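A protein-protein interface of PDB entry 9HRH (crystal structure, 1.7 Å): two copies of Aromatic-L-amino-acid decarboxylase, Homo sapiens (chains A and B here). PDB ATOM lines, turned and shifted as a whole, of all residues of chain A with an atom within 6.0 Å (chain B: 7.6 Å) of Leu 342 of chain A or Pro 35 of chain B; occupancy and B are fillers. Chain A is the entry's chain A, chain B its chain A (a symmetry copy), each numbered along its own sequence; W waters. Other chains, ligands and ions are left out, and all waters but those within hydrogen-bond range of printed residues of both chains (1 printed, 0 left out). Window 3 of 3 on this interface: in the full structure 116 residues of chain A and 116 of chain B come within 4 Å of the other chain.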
ATOM      1  N   TRP A 105     -17.952 -25.487   6.539  1.00  0.00           N
ATOM      2  CA  TRP A 105     -16.603 -25.038   6.213  1.00  0.00           C
ATOM      3  C   TRP A 105     -16.349 -23.640   6.762  1.00  0.00           C
ATOM      4  O   TRP A 105     -15.274 -23.361   7.303  1.00  0.00           O
ATOM      5  CB  TRP A 105     -16.388 -25.070   4.699  1.00  0.00           C
ATOM      6  CG  TRP A 105     -15.028 -24.601   4.270  1.00  0.00           C
ATOM      7  CD1 TRP A 105     -13.916 -25.373   4.093  1.00  0.00           C
ATOM      8  CD2 TRP A 105     -14.636 -23.256   3.964  1.00  0.00           C
ATOM      9  NE1 TRP A 105     -12.856 -24.594   3.695  1.00  0.00           N
ATOM     10  CE2 TRP A 105     -13.272 -23.290   3.608  1.00  0.00           C
ATOM     11  CE3 TRP A 105     -15.303 -22.028   3.958  1.00  0.00           C
ATOM     12  CZ2 TRP A 105     -12.565 -22.143   3.250  1.00  0.00           C
ATOM     13  CZ3 TRP A 105     -14.600 -20.889   3.602  1.00  0.00           C
ATOM     14  CH2 TRP A 105     -13.244 -20.956   3.253  1.00  0.00           C
ATOM     15  N   GLU A 113     -10.668 -28.951   6.535  1.00  0.00           N
ATOM     16  CA  GLU A 113      -9.639 -29.255   5.544  1.00  0.00           C
ATOM     17  C   GLU A 113      -8.575 -30.195   6.099  1.00  0.00           C
ATOM     18  O   GLU A 113      -8.115 -31.100   5.394  1.00  0.00           O
ATOM     19  CB  GLU A 113      -9.009 -27.960   5.038  1.00  0.00           C
ATOM     20  CG  GLU A 113     -10.027 -26.991   4.460  1.00  0.00           C
ATOM     21  CD  GLU A 113      -9.526 -26.296   3.217  1.00  0.00           C
ATOM     22  OE1 GLU A 113      -8.408 -26.621   2.768  1.00  0.00           O
ATOM     23  OE2 GLU A 113     -10.254 -25.430   2.686  1.00  0.00           O
ATOM     24  N   ASN A 134      -9.941 -39.077  -1.123  1.00  0.00           N
ATOM     25  CA  ASN A 134     -10.487 -37.832  -1.651  1.00  0.00           C
ATOM     26  C   ASN A 134      -9.531 -37.105  -2.587  1.00  0.00           C
ATOM     27  O   ASN A 134      -9.986 -36.353  -3.457  1.00  0.00           O
ATOM     28  CB  ASN A 134     -10.874 -36.897  -0.504  1.00  0.00           C
ATOM     29  CG  ASN A 134     -11.526 -35.620  -0.991  1.00  0.00           C
ATOM     30  OD1 ASN A 134     -12.717 -35.594  -1.300  1.00  0.00           O
ATOM     31  ND2 ASN A 134     -10.743 -34.552  -1.072  1.00  0.00           N
ATOM     32  N   ALA A 137      -9.535 -35.340  -7.050  1.00  0.00           N
ATOM     33  CA  ALA A 137     -10.904 -35.275  -7.574  1.00  0.00           C
ATOM     34  C   ALA A 137     -11.610 -36.630  -7.594  1.00  0.00           C
ATOM     35  O   ALA A 137     -12.485 -36.864  -8.432  1.00  0.00           O
ATOM     36  CB  ALA A 137     -10.923 -34.661  -8.975  1.00  0.00           C
ATOM     37  N   ARG A 319     -19.244 -40.208  -2.148  1.00  0.00           N
ATOM     38  CA  ARG A 319     -19.700 -39.272  -1.126  1.00  0.00           C
ATOM     39  C   ARG A 319     -21.142 -38.841  -1.356  1.00  0.00           C
ATOM     40  O   ARG A 319     -21.840 -38.486  -0.400  1.00  0.00           O
ATOM     41  CB  ARG A 319     -18.781 -38.050  -1.088  1.00  0.00           C
ATOM     42  CG  ARG A 319     -17.302 -38.395  -1.008  1.00  0.00           C
ATOM     43  CD  ARG A 319     -16.434 -37.149  -1.027  1.00  0.00           C
ATOM     44  NE  ARG A 319     -16.754 -36.284  -2.155  1.00  0.00           N
ATOM     45  CZ  ARG A 319     -15.925 -36.031  -3.156  1.00  0.00           C
ATOM     46  NH1 ARG A 319     -14.715 -36.564  -3.202  1.00  0.00           N
ATOM     47  NH2 ARG A 319     -16.320 -35.225  -4.137  1.00  0.00           N
ATOM     48  N   LEU A 342     -13.686 -31.626  -3.916  1.00  0.00           N
ATOM     49  CA  LEU A 342     -13.420 -30.916  -2.670  1.00  0.00           C
ATOM     50  C   LEU A 342     -14.534 -31.111  -1.649  1.00  0.00           C
ATOM     51  O   LEU A 342     -15.708 -30.884  -1.942  1.00  0.00           O
ATOM     52  CB  LEU A 342     -13.229 -29.423  -2.934  1.00  0.00           C
ATOM     53  CG  LEU A 342     -13.018 -28.560  -1.690  1.00  0.00           C
ATOM     54  CD1 LEU A 342     -11.743 -28.945  -0.952  1.00  0.00           C
ATOM     55  CD2 LEU A 342     -12.988 -27.103  -2.090  1.00  0.00           C
ATOM     56  N   ILE A 343     -14.156 -31.539  -0.449  1.00  0.00           N
ATOM     57  CA  ILE A 343     -15.093 -31.672   0.659  1.00  0.00           C
ATOM     58  C   ILE A 343     -15.127 -30.354   1.422  1.00  0.00           C
ATOM     59  O   ILE A 343     -14.115 -29.928   1.987  1.00  0.00           O
ATOM     60  CB  ILE A 343     -14.703 -32.831   1.588  1.00  0.00           C
ATOM     61  CG1 ILE A 343     -14.733 -34.164   0.836  1.00  0.00           C
ATOM     62  CG2 ILE A 343     -15.621 -32.861   2.800  1.00  0.00           C
ATOM     63  CD1 ILE A 343     -14.179 -35.320   1.637  1.00  0.00           C
ATOM     64  N   THR A 344     -16.288 -29.709   1.437  1.00  0.00           N
ATOM     65  CA  THR A 344     -16.496 -28.498   2.222  1.00  0.00           C
ATOM     66  C   THR A 344     -17.395 -28.716   3.427  1.00  0.00           C
ATOM     67  O   THR A 344     -17.156 -28.126   4.483  1.00  0.00           O
ATOM     68  CB  THR A 344     -17.088 -27.386   1.348  1.00  0.00           C
ATOM     69  OG1 THR A 344     -18.051 -27.944   0.444  1.00  0.00           O
ATOM     70  CG2 THR A 344     -15.991 -26.688   0.556  1.00  0.00           C
ATOM     71  N   ASP B  32      -9.391 -15.347   5.745  1.00  0.00           N
ATOM     72  CA  ASP B  32      -9.341 -14.955   4.343  1.00  0.00           C
ATOM     73  C   ASP B  32      -9.007 -16.114   3.417  1.00  0.00           C
ATOM     74  O   ASP B  32      -8.892 -15.907   2.203  1.00  0.00           O
ATOM     75  CB  ASP B  32      -8.318 -13.832   4.145  1.00  0.00           C
ATOM     76  CG  ASP B  32      -8.891 -12.459   4.438  1.00  0.00           C
ATOM     77  OD1 ASP B  32      -8.295 -11.733   5.260  1.00  0.00           O
ATOM     78  OD2 ASP B  32      -9.929 -12.103   3.842  1.00  0.00           O
ATOM     79  N   VAL B  33      -8.841 -17.327   3.951  1.00  0.00           N
ATOM     80  CA  VAL B  33      -8.548 -18.472   3.099  1.00  0.00           C
ATOM     81  C   VAL B  33      -9.778 -18.837   2.274  1.00  0.00           C
ATOM     82  O   VAL B  33     -10.918 -18.483   2.599  1.00  0.00           O
ATOM     83  CB  VAL B  33      -8.067 -19.673   3.932  1.00  0.00           C
ATOM     84  CG1 VAL B  33      -6.797 -19.326   4.690  1.00  0.00           C
ATOM     85  CG2 VAL B  33      -9.162 -20.132   4.887  1.00  0.00           C
ATOM     86  N   GLU B  34      -9.537 -19.551   1.184  1.00  0.00           N
ATOM     87  CA  GLU B  34     -10.586 -20.092   0.339  1.00  0.00           C
ATOM     88  C   GLU B  34     -10.611 -21.613   0.436  1.00  0.00           C
ATOM     89  O   GLU B  34      -9.628 -22.233   0.855  1.00  0.00           O
ATOM     90  CB  GLU B  34     -10.384 -19.657  -1.119  1.00  0.00           C
ATOM     91  CG  GLU B  34     -10.374 -18.148  -1.299  1.00  0.00           C
ATOM     92  CD  GLU B  34     -11.769 -17.554  -1.231  1.00  0.00           C
ATOM     93  OE1 GLU B  34     -12.748 -18.321  -1.355  1.00  0.00           O
ATOM     94  OE2 GLU B  34     -11.889 -16.324  -1.051  1.00  0.00           O
ATOM     95  N   PRO B  35     -11.732 -22.246   0.088  1.00  0.00           N
ATOM     96  CA  PRO B  35     -11.835 -23.703   0.228  1.00  0.00           C
ATOM     97  C   PRO B  35     -10.713 -24.439  -0.490  1.00  0.00           C
ATOM     98  O   PRO B  35     -10.447 -24.209  -1.672  1.00  0.00           O
ATOM     99  CB  PRO B  35     -13.202 -24.004  -0.388  1.00  0.00           C
ATOM    100  CG  PRO B  35     -14.000 -22.805  -0.022  1.00  0.00           C
ATOM    101  CD  PRO B  35     -13.039 -21.658  -0.262  1.00  0.00           C
ATOM    102  N   GLY B  36     -10.047 -25.325   0.248  1.00  0.00           N
ATOM    103  CA  GLY B  36      -8.959 -26.114  -0.285  1.00  0.00           C
ATOM    104  C   GLY B  36      -7.578 -25.525  -0.097  1.00  0.00           C
ATOM    105  O   GLY B  36      -6.652 -25.928  -0.809  1.00  0.00           O
ATOM    106  N   TYR B  37      -7.399 -24.595   0.848  1.00  0.00           N
ATOM    107  CA  TYR B  37      -6.124 -23.890   0.918  1.00  0.00           C
ATOM    108  C   TYR B  37      -5.058 -24.773   1.541  1.00  0.00           C
ATOM    109  O   TYR B  37      -3.862 -24.576   1.296  1.00  0.00           O
ATOM    110  CB  TYR B  37      -6.232 -22.618   1.766  1.00  0.00           C
ATOM    111  CG  TYR B  37      -6.265 -22.887   3.262  1.00  0.00           C
ATOM    112  CD1 TYR B  37      -7.443 -23.166   3.938  1.00  0.00           C
ATOM    113  CD2 TYR B  37      -5.086 -22.811   4.001  1.00  0.00           C
ATOM    114  CE1 TYR B  37      -7.436 -23.403   5.310  1.00  0.00           C
ATOM    115  CE2 TYR B  37      -5.072 -23.041   5.356  1.00  0.00           C
ATOM    116  CZ  TYR B  37      -6.240 -23.335   6.009  1.00  0.00           C
ATOM    117  OH  TYR B  37      -6.194 -23.556   7.365  1.00  0.00           O
ATOM    118  N   LEU B  38      -5.480 -25.736   2.366  1.00  0.00           N
ATOM    119  CA  LEU B  38      -4.571 -26.416   3.285  1.00  0.00           C
ATOM    120  C   LEU B  38      -3.783 -27.526   2.606  1.00  0.00           C
ATOM    121  O   LEU B  38      -2.591 -27.695   2.886  1.00  0.00           O
ATOM    122  CB  LEU B  38      -5.350 -26.980   4.472  1.00  0.00           C
ATOM    123  CG  LEU B  38      -4.492 -27.484   5.636  1.00  0.00           C
ATOM    124  CD1 LEU B  38      -3.528 -26.399   6.087  1.00  0.00           C
ATOM    125  CD2 LEU B  38      -5.367 -27.939   6.791  1.00  0.00           C
ATOM    126  N   ARG B  39      -4.428 -28.294   1.728  1.00  0.00           N
ATOM    127  CA  ARG B  39      -3.748 -29.413   1.081  1.00  0.00           C
ATOM    128  C   ARG B  39      -2.414 -29.043   0.439  1.00  0.00           C
ATOM    129  O   ARG B  39      -1.448 -29.803   0.626  1.00  0.00           O
ATOM    130  CB  ARG B  39      -4.674 -30.069   0.044  1.00  0.00           C
ATOM    131  CG  ARG B  39      -4.207 -31.446  -0.412  1.00  0.00           C
ATOM    132  CD  ARG B  39      -5.134 -32.037  -1.463  1.00  0.00           C
ATOM    133  NE  ARG B  39      -6.383 -32.528  -0.896  1.00  0.00           N
ATOM    134  CZ  ARG B  39      -6.529 -33.695  -0.281  1.00  0.00           C
ATOM    135  NH1 ARG B  39      -5.510 -34.525  -0.119  1.00  0.00           N
ATOM    136  NH2 ARG B  39      -7.727 -34.041   0.180  1.00  0.00           N
HETATM  137  O   HOH W   1      -7.433 -28.703   1.467  1.00  0.00           O
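OE2 of Glu 113 of chain A lies within hydrogen-bond range of N of Gly 36 of chain B (2.4 Å).
The backbone NH (N) of Tyr 37 of chain B is in hydrogen-bond range of the side-chain carboxylate (OE1) of Glu 113 of chain A.
OE1 of Glu 113 of chain A sits at hydrogen-bond distance from N of Leu 38 of chain B (3.1 Å).
The side-chain amide nitrogen of Asn 134 of chain A sits close to the guanidinium group of Arg 39 of chain B (3.3 Å).
NE1 of Trp 105 of chain A is in hydrogen-bond range of OE2 of Glu 113 of chain A.
The backbone NH of Trp 105 of chain A sits close to the backbone carbonyl oxygen of Thr 344 of chain A, at 3.4 Å.
The side-chain amide oxygen of Asn 134 of chain A is in hydrogen-bond range of the guanidinium group of Arg 319 of chain A (2.9 Å).
Among the printed residues, pairs that only touch across the chains: Trp 105 of chain A with Val 33 of chain B (3.5 Å), Trp 105 of chain A with Glu 34 of chain B (3.5 Å), Trp 105 of chain A with Pro 35 of chain B (3.3 Å), Glu 113 of chain A with Glu 34 of chain B (3.7 Å), Glu 113 of chain A with Pro 35 of chain B (3.4 Å), Leu 342 of chain A with Pro 35 of chain B (3.5 Å) and Thr 344 of chain A with Pro 35 of chain B (3.98 Å).
Leu 342 of chain A touches one residue of chain B.
Printed residues of chain A within 4 Å of Pro 35 of chain B: Trp 105 (3.3 Å), Glu 113 (3.4 Å), Leu 342 (3.5 Å) and Thr 344 (3.98 Å).
Of the printed residues of chain A, Tyr 37 of chain B touches Glu 113 (3.0 Å).
Printed residues of chain B within 4 Å of Thr 344 of chain A: Pro 35.
Printed residues of chain B within 4 Å of Glu 113 of chain A: Glu 34, Pro 35, Gly 36, Tyr 37 and Leu 38.
Of the printed residues of chain A, Gly 36 of chain B touches Glu 113.
Ala 137 of chain A touches none of the printed residues of chain B.
The nearest printed residue of chain A that does not touch Glu 34 of chain B is Leu 342 of chain A (6.5 Å).
Printed residues of chain A that touch a printed residue of chain B: Trp 105, Glu 113, Asn 134, Leu 342 and Thr 344.
Hydrophobic or aromatic side chains of chain A that line the printed part of chain B: Trp 105 and Leu 342.
Printed residues of chain B that touch a printed residue of chain A: Val 33, Glu 34, Pro 35, Gly 36, Tyr 37, Leu 38 and Arg 39.
Among the printed residues, 11 pairs touch across the chains.
Among the printed residues, no Asp or Glu carboxylate lies within 4 Å of a Lys or Arg side-chain nitrogen of the other chain.
No position is printed for both chains.
Of the 11 pairs that touch across the chains among the printed residues, none has its exchanged pair printed and touching as well.
Water W1 lies within hydrogen-bond range of OE1 of Glu 113 of chain A (2.6 Å) and N of Arg 39 of chain B (3.0 Å).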
